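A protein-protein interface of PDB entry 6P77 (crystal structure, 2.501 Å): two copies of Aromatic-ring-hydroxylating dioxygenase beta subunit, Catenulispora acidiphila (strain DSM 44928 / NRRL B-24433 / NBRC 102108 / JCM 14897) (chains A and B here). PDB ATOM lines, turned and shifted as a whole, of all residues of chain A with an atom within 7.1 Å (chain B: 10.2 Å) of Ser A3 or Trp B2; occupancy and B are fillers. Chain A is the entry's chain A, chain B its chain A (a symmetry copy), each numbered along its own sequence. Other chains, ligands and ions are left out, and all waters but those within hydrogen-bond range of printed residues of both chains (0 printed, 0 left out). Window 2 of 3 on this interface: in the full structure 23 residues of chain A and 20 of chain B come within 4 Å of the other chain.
The backbone NH of Ser A3 lies close to a ring nitrogen (ND1) of His A1 (3.2 Å).
The indole nitrogen (NE1) of Trp B2 sits at hydrogen-bond distance from the side-chain hydroxyl (OG) of Ser A3, 3.2 Å away.
Printed residues of chain B that touch a printed residue of chain A: Trp B2, Ala B5 and Tyr B8. Printed residues of chain A that touch a printed residue of chain B: Trp A2, Ser A3, Ala A6 and Ala A9. Hydrophobic or aromatic side chains of chain A that line the printed part of chain B: Trp A2, Ala A6 and Ala A9. Among the printed residues, 4 pairs touch across the chains.
O of Trp A2 touches CD1 of Trp B2, at 3.6 Å. Ala A6 touches Ala B5 (CA to CB, 3.5 Å). Ala A9 touches Tyr B8 (CB to CD1, 3.99 Å).
Trp A2 touches its own counterpart, Trp B2. Ser A3 touches Trp B2, but with the chains exchanged Trp A2 does not touch Ser B3 (7.7 Å). Ala A6 touches Ala B5, but with the chains exchanged Ala A5 does not touch Ala B6 (7.0 Å). Ala A9 touches Tyr B8, but with the chains exchanged Tyr A8 does not touch Ala B9 (8.3 Å). Of the 4 pairs that touch across the chains among the printed residues, 1 has its exchanged pair printed and touching as well.
No residue of chain B comes within 4 Å of His A1. No residue of chain B comes within 4 Å of Ala A5. Ala A6 touches one residue of chain B. No residue of chain B comes within 4 Å of Leu A7. Of the printed residues of chain B, Ala A9 touches Tyr B8. Trp B2 touches two residues of chain A. Of the printed residues of chain A, Ala B5 touches Ala A6 (3.5 Å). Of the printed residues of chain A, Tyr B8 touches Ala A9 (3.99 Å). The nearest residue of chain A that does not touch Trp B2 is Ala A6 (4.1 Å). The nearest printed residue of chain A that does not touch Tyr B8 is Tyr A8 (6.0 Å).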
ATOM      1  N   HIS A   1      -7.628  27.503   4.030  1.00  0.00           N
ATOM      2  CA  HIS A   1      -7.717  26.635   2.832  1.00  0.00           C
ATOM      3  C   HIS A   1      -6.575  25.604   2.789  1.00  0.00           C
ATOM      4  O   HIS A   1      -5.394  25.873   3.131  1.00  0.00           O
ATOM      5  CB  HIS A   1      -7.738  27.450   1.539  1.00  0.00           C
ATOM      6  CG  HIS A   1      -8.673  26.912   0.501  1.00  0.00           C
ATOM      7  ND1 HIS A   1      -8.312  25.917  -0.386  1.00  0.00           N
ATOM      8  CD2 HIS A   1      -9.955  27.229   0.209  1.00  0.00           C
ATOM      9  CE1 HIS A   1      -9.330  25.649  -1.182  1.00  0.00           C
ATOM     10  NE2 HIS A   1     -10.338  26.435  -0.844  1.00  0.00           N
ATOM     11  N   TRP A   2      -6.967  24.392   2.384  1.00  0.00           N
ATOM     12  CA  TRP A   2      -6.054  23.278   2.210  1.00  0.00           C
ATOM     13  C   TRP A   2      -5.072  23.590   1.067  1.00  0.00           C
ATOM     14  O   TRP A   2      -3.912  23.191   1.160  1.00  0.00           O
ATOM     15  CB  TRP A   2      -6.807  21.968   1.969  1.00  0.00           C
ATOM     16  CG  TRP A   2      -7.727  21.530   3.106  1.00  0.00           C
ATOM     17  CD1 TRP A   2      -7.493  21.641   4.454  1.00  0.00           C
ATOM     18  CD2 TRP A   2      -9.011  20.873   2.975  1.00  0.00           C
ATOM     19  NE1 TRP A   2      -8.550  21.101   5.163  1.00  0.00           N
ATOM     20  CE2 TRP A   2      -9.490  20.626   4.285  1.00  0.00           C
ATOM     21  CE3 TRP A   2      -9.787  20.465   1.881  1.00  0.00           C
ATOM     22  CZ2 TRP A   2     -10.713  19.998   4.529  1.00  0.00           C
ATOM     23  CZ3 TRP A   2     -11.019  19.851   2.124  1.00  0.00           C
ATOM     24  CH2 TRP A   2     -11.465  19.623   3.441  1.00  0.00           C
ATOM     25  N   SER A   3      -5.520  24.340   0.044  1.00  0.00           N
ATOM     26  CA  SER A   3      -4.665  24.749  -1.089  1.00  0.00           C
ATOM     27  C   SER A   3      -3.570  25.771  -0.742  1.00  0.00           C
ATOM     28  O   SER A   3      -2.448  25.661  -1.243  1.00  0.00           O
ATOM     29  CB  SER A   3      -5.508  25.260  -2.266  1.00  0.00           C
ATOM     30  OG  SER A   3      -6.328  24.209  -2.760  1.00  0.00           O
ATOM     31  N   GLN A   4      -3.919  26.759   0.093  1.00  0.00           N
ATOM     32  CA  GLN A   4      -2.977  27.729   0.655  1.00  0.00           C
ATOM     33  C   GLN A   4      -1.876  26.963   1.404  1.00  0.00           C
ATOM     34  O   GLN A   4      -0.675  27.209   1.215  1.00  0.00           O
ATOM     35  CB  GLN A   4      -3.678  28.624   1.683  1.00  0.00           C
ATOM     36  CG  GLN A   4      -3.959  30.059   1.323  1.00  0.00           C
ATOM     37  CD  GLN A   4      -4.646  30.793   2.488  1.00  0.00           C
ATOM     38  OE1 GLN A   4      -4.075  31.042   3.612  1.00  0.00           O
ATOM     39  NE2 GLN A   4      -5.890  31.136   2.241  1.00  0.00           N
ATOM     40  N   ALA A   5      -2.303  26.015   2.252  1.00  0.00           N
ATOM     41  CA  ALA A   5      -1.375  25.224   3.038  1.00  0.00           C
ATOM     42  C   ALA A   5      -0.495  24.411   2.135  1.00  0.00           C
ATOM     43  O   ALA A   5       0.725  24.363   2.335  1.00  0.00           O
ATOM     44  CB  ALA A   5      -2.127  24.317   3.971  1.00  0.00           C
ATOM     45  N   ALA A   6      -1.115  23.762   1.137  1.00  0.00           N
ATOM     46  CA  ALA A   6      -0.367  22.945   0.192  1.00  0.00           C
ATOM     47  C   ALA A   6       0.666  23.792  -0.535  1.00  0.00           C
ATOM     48  O   ALA A   6       1.812  23.360  -0.713  1.00  0.00           O
ATOM     49  CB  ALA A   6      -1.269  22.224  -0.777  1.00  0.00           C
ATOM     50  N   LEU A   7       0.289  25.023  -0.902  1.00  0.00           N
ATOM     51  CA  LEU A   7       1.220  25.927  -1.586  1.00  0.00           C
ATOM     52  C   LEU A   7       2.436  26.271  -0.693  1.00  0.00           C
ATOM     53  O   LEU A   7       3.579  26.348  -1.149  1.00  0.00           O
ATOM     54  CB  LEU A   7       0.495  27.213  -1.999  1.00  0.00           C
ATOM     55  CG  LEU A   7       1.352  28.259  -2.735  1.00  0.00           C
ATOM     56  CD1 LEU A   7       1.914  27.674  -4.034  1.00  0.00           C
ATOM     57  CD2 LEU A   7       0.559  29.529  -3.019  1.00  0.00           C
ATOM     58  N   TYR A   8       2.164  26.495   0.592  1.00  0.00           N
ATOM     59  CA  TYR A   8       3.203  26.835   1.546  1.00  0.00           C
ATOM     60  C   TYR A   8       4.295  25.726   1.619  1.00  0.00           C
ATOM     61  O   TYR A   8       5.498  26.013   1.571  1.00  0.00           O
ATOM     62  CB  TYR A   8       2.557  27.126   2.901  1.00  0.00           C
ATOM     63  CG  TYR A   8       3.466  27.792   3.899  1.00  0.00           C
ATOM     64  CD1 TYR A   8       4.255  27.041   4.748  1.00  0.00           C
ATOM     65  CD2 TYR A   8       3.495  29.170   4.022  1.00  0.00           C
ATOM     66  CE1 TYR A   8       5.098  27.628   5.658  1.00  0.00           C
ATOM     67  CE2 TYR A   8       4.344  29.780   4.932  1.00  0.00           C
ATOM     68  CZ  TYR A   8       5.140  28.991   5.744  1.00  0.00           C
ATOM     69  OH  TYR A   8       5.948  29.571   6.649  1.00  0.00           O
ATOM     70  N   ALA A   9       3.845  24.472   1.737  1.00  0.00           N
ATOM     71  CA  ALA A   9       4.725  23.291   1.762  1.00  0.00           C
ATOM     72  C   ALA A   9       5.452  23.164   0.434  1.00  0.00           C
ATOM     73  O   ALA A   9       6.639  22.872   0.364  1.00  0.00           O
ATOM     74  CB  ALA A   9       3.931  22.019   2.031  1.00  0.00           C
ATOM     75  N   GLU A  10       4.726  23.418  -0.639  1.00  0.00           N
ATOM     76  CA  GLU A  10       5.324  23.348  -1.949  1.00  0.00           C
ATOM     77  C   GLU A  10       6.502  24.338  -2.094  1.00  0.00           C
ATOM     78  O   GLU A  10       7.541  24.011  -2.640  1.00  0.00           O
ATOM     79  CB  GLU A  10       4.254  23.545  -3.022  1.00  0.00           C
ATOM     80  CG  GLU A  10       4.659  22.891  -4.314  1.00  0.00           C
ATOM     81  CD  GLU A  10       3.724  23.181  -5.468  1.00  0.00           C
ATOM     82  OE1 GLU A  10       2.572  23.621  -5.243  1.00  0.00           O
ATOM     83  OE2 GLU A  10       4.205  22.986  -6.594  1.00  0.00           O
ATOM     84  N   ILE A  82       4.154  33.861   2.649  1.00  0.00           N
ATOM     85  CA  ILE A  82       3.769  33.966   1.264  1.00  0.00           C
ATOM     86  C   ILE A  82       2.540  34.829   1.144  1.00  0.00           C
ATOM     87  O   ILE A  82       1.807  35.008   2.133  1.00  0.00           O
ATOM     88  CB  ILE A  82       3.578  32.589   0.577  1.00  0.00           C
ATOM     89  CG1 ILE A  82       2.427  31.828   1.174  1.00  0.00           C
ATOM     90  CG2 ILE A  82       4.839  31.753   0.707  1.00  0.00           C
ATOM     91  CD1 ILE A  82       2.109  30.559   0.421  1.00  0.00           C
ATOM     92  N   HIS B   1      -0.891  18.044  -4.529  1.00  0.00           N
ATOM     93  CA  HIS B   1      -1.784  17.218  -3.683  1.00  0.00           C
ATOM     94  C   HIS B   1      -1.769  17.683  -2.216  1.00  0.00           C
ATOM     95  O   HIS B   1      -0.722  18.062  -1.628  1.00  0.00           O
ATOM     96  CB  HIS B   1      -1.437  15.732  -3.767  1.00  0.00           C
ATOM     97  CG  HIS B   1      -2.632  14.832  -3.787  1.00  0.00           C
ATOM     98  ND1 HIS B   1      -3.261  14.398  -2.637  1.00  0.00           N
ATOM     99  CD2 HIS B   1      -3.315  14.284  -4.819  1.00  0.00           C
ATOM    100  CE1 HIS B   1      -4.276  13.619  -2.960  1.00  0.00           C
ATOM    101  NE2 HIS B   1      -4.328  13.531  -4.278  1.00  0.00           N
ATOM    102  N   TRP B   2      -2.975  17.675  -1.641  1.00  0.00           N
ATOM    103  CA  TRP B   2      -3.195  18.016  -0.248  1.00  0.00           C
ATOM    104  C   TRP B   2      -2.510  16.975   0.652  1.00  0.00           C
ATOM    105  O   TRP B   2      -2.002  17.350   1.708  1.00  0.00           O
ATOM    106  CB  TRP B   2      -4.686  18.147   0.068  1.00  0.00           C
ATOM    107  CG  TRP B   2      -5.422  19.236  -0.711  1.00  0.00           C
ATOM    108  CD1 TRP B   2      -4.950  20.480  -1.045  1.00  0.00           C
ATOM    109  CD2 TRP B   2      -6.780  19.175  -1.209  1.00  0.00           C
ATOM    110  NE1 TRP B   2      -5.925  21.189  -1.723  1.00  0.00           N
ATOM    111  CE2 TRP B   2      -7.051  20.414  -1.837  1.00  0.00           C
ATOM    112  CE3 TRP B   2      -7.785  18.198  -1.174  1.00  0.00           C
ATOM    113  CZ2 TRP B   2      -8.282  20.699  -2.432  1.00  0.00           C
ATOM    114  CZ3 TRP B   2      -9.012  18.476  -1.783  1.00  0.00           C
ATOM    115  CH2 TRP B   2      -9.247  19.720  -2.401  1.00  0.00           C
ATOM    116  N   SER B   3      -2.448  15.706   0.208  1.00  0.00           N
ATOM    117  CA  SER B   3      -1.777  14.624   0.956  1.00  0.00           C
ATOM    118  C   SER B   3      -0.245  14.735   1.027  1.00  0.00           C
ATOM    119  O   SER B   3       0.342  14.453   2.075  1.00  0.00           O
ATOM    120  CB  SER B   3      -2.179  13.244   0.416  1.00  0.00           C
ATOM    121  OG  SER B   3      -3.573  13.041   0.610  1.00  0.00           O
ATOM    122  N   GLN B   4       0.378  15.124  -0.094  1.00  0.00           N
ATOM    123  CA  GLN B   4       1.807  15.434  -0.173  1.00  0.00           C
ATOM    124  C   GLN B   4       2.124  16.538   0.847  1.00  0.00           C
ATOM    125  O   GLN B   4       3.075  16.433   1.637  1.00  0.00           O
ATOM    126  CB  GLN B   4       2.160  15.988  -1.558  1.00  0.00           C
ATOM    127  CG  GLN B   4       2.943  15.122  -2.508  1.00  0.00           C
ATOM    128  CD  GLN B   4       3.213  15.861  -3.830  1.00  0.00           C
ATOM    129  OE1 GLN B   4       3.971  16.895  -3.928  1.00  0.00           O
ATOM    130  NE2 GLN B   4       2.582  15.351  -4.863  1.00  0.00           N
ATOM    131  N   ALA B   5       1.302  17.598   0.829  1.00  0.00           N
ATOM    132  CA  ALA B   5       1.492  18.723   1.726  1.00  0.00           C
ATOM    133  C   ALA B   5       1.340  18.279   3.151  1.00  0.00           C
ATOM    134  O   ALA B   5       2.159  18.640   4.006  1.00  0.00           O
ATOM    135  CB  ALA B   5       0.496  19.805   1.418  1.00  0.00           C
ATOM    136  N   ALA B   6       0.283  17.495   3.414  1.00  0.00           N
ATOM    137  CA  ALA B   6       0.031  16.995   4.758  1.00  0.00           C
ATOM    138  C   ALA B   6       1.208  16.162   5.240  1.00  0.00           C
ATOM    139  O   ALA B   6       1.636  16.295   6.394  1.00  0.00           O
ATOM    140  CB  ALA B   6      -1.262  16.228   4.850  1.00  0.00           C
ATOM    141  N   LEU B   7       1.778  15.347   4.344  1.00  0.00           N
ATOM    142  CA  LEU B   7       2.936  14.520   4.703  1.00  0.00           C
ATOM    143  C   LEU B   7       4.155  15.389   5.093  1.00  0.00           C
ATOM    144  O   LEU B   7       4.899  15.088   6.029  1.00  0.00           O
ATOM    145  CB  LEU B   7       3.304  13.597   3.535  1.00  0.00           C
ATOM    146  CG  LEU B   7       4.505  12.663   3.772  1.00  0.00           C
ATOM    147  CD1 LEU B   7       4.235  11.731   4.956  1.00  0.00           C
ATOM    148  CD2 LEU B   7       4.838  11.858   2.522  1.00  0.00           C
ATOM    149  N   TYR B   8       4.357  16.470   4.341  1.00  0.00           N
ATOM    150  CA  TYR B   8       5.466  17.375   4.584  1.00  0.00           C
ATOM    151  C   TYR B   8       5.413  17.968   6.024  1.00  0.00           C
ATOM    152  O   TYR B   8       6.419  17.980   6.745  1.00  0.00           O
ATOM    153  CB  TYR B   8       5.478  18.449   3.497  1.00  0.00           C
ATOM    154  CG  TYR B   8       6.742  19.265   3.435  1.00  0.00           C
ATOM    155  CD1 TYR B   8       6.878  20.416   4.185  1.00  0.00           C
ATOM    156  CD2 TYR B   8       7.775  18.907   2.587  1.00  0.00           C
ATOM    157  CE1 TYR B   8       8.025  21.169   4.151  1.00  0.00           C
ATOM    158  CE2 TYR B   8       8.943  19.652   2.544  1.00  0.00           C
ATOM    159  CZ  TYR B   8       9.050  20.782   3.334  1.00  0.00           C
ATOM    160  OH  TYR B   8      10.168  21.528   3.281  1.00  0.00           O
ATOM    161  N   ALA B   9       4.228  18.452   6.411  1.00  0.00           N
ATOM    162  CA  ALA B   9       3.972  18.998   7.755  1.00  0.00           C
ATOM    163  C   ALA B   9       4.138  17.902   8.794  1.00  0.00           C
ATOM    164  O   ALA B   9       4.711  18.092   9.859  1.00  0.00           O
ATOM    165  CB  ALA B   9       2.569  19.584   7.852  1.00  0.00           C
ATOM    166  N   GLU B  10       3.646  16.723   8.462  1.00  0.00           N
ATOM    167  CA  GLU B  10       3.769  15.607   9.367  1.00  0.00           C
ATOM    168  C   GLU B  10       5.249  15.284   9.678  1.00  0.00           C
ATOM    169  O   GLU B  10       5.615  15.025  10.811  1.00  0.00           O
ATOM    170  CB  GLU B  10       3.006  14.403   8.817  1.00  0.00           C
ATOM    171  CG  GLU B  10       2.582  13.481   9.926  1.00  0.00           C
ATOM    172  CD  GLU B  10       1.963  12.187   9.445  1.00  0.00           C
ATOM    173  OE1 GLU B  10       1.546  12.094   8.267  1.00  0.00           O
ATOM    174  OE2 GLU B  10       1.949  11.270  10.281  1.00  0.00           O
ATOM    175  N   ILE B  82      11.359  16.095   0.695  1.00  0.00           N
ATOM    176  CA  ILE B  82      10.935  14.722   0.802  1.00  0.00           C
ATOM    177  C   ILE B  82      10.711  14.152  -0.574  1.00  0.00           C
ATOM    178  O   ILE B  82      10.520  14.914  -1.539  1.00  0.00           O
ATOM    179  CB  ILE B  82       9.696  14.534   1.714  1.00  0.00           C
ATOM    180  CG1 ILE B  82       8.478  15.202   1.137  1.00  0.00           C
ATOM    181  CG2 ILE B  82       9.962  15.108   3.095  1.00  0.00           C
ATOM    182  CD1 ILE B  82       7.219  14.900   1.914  1.00  0.00           C
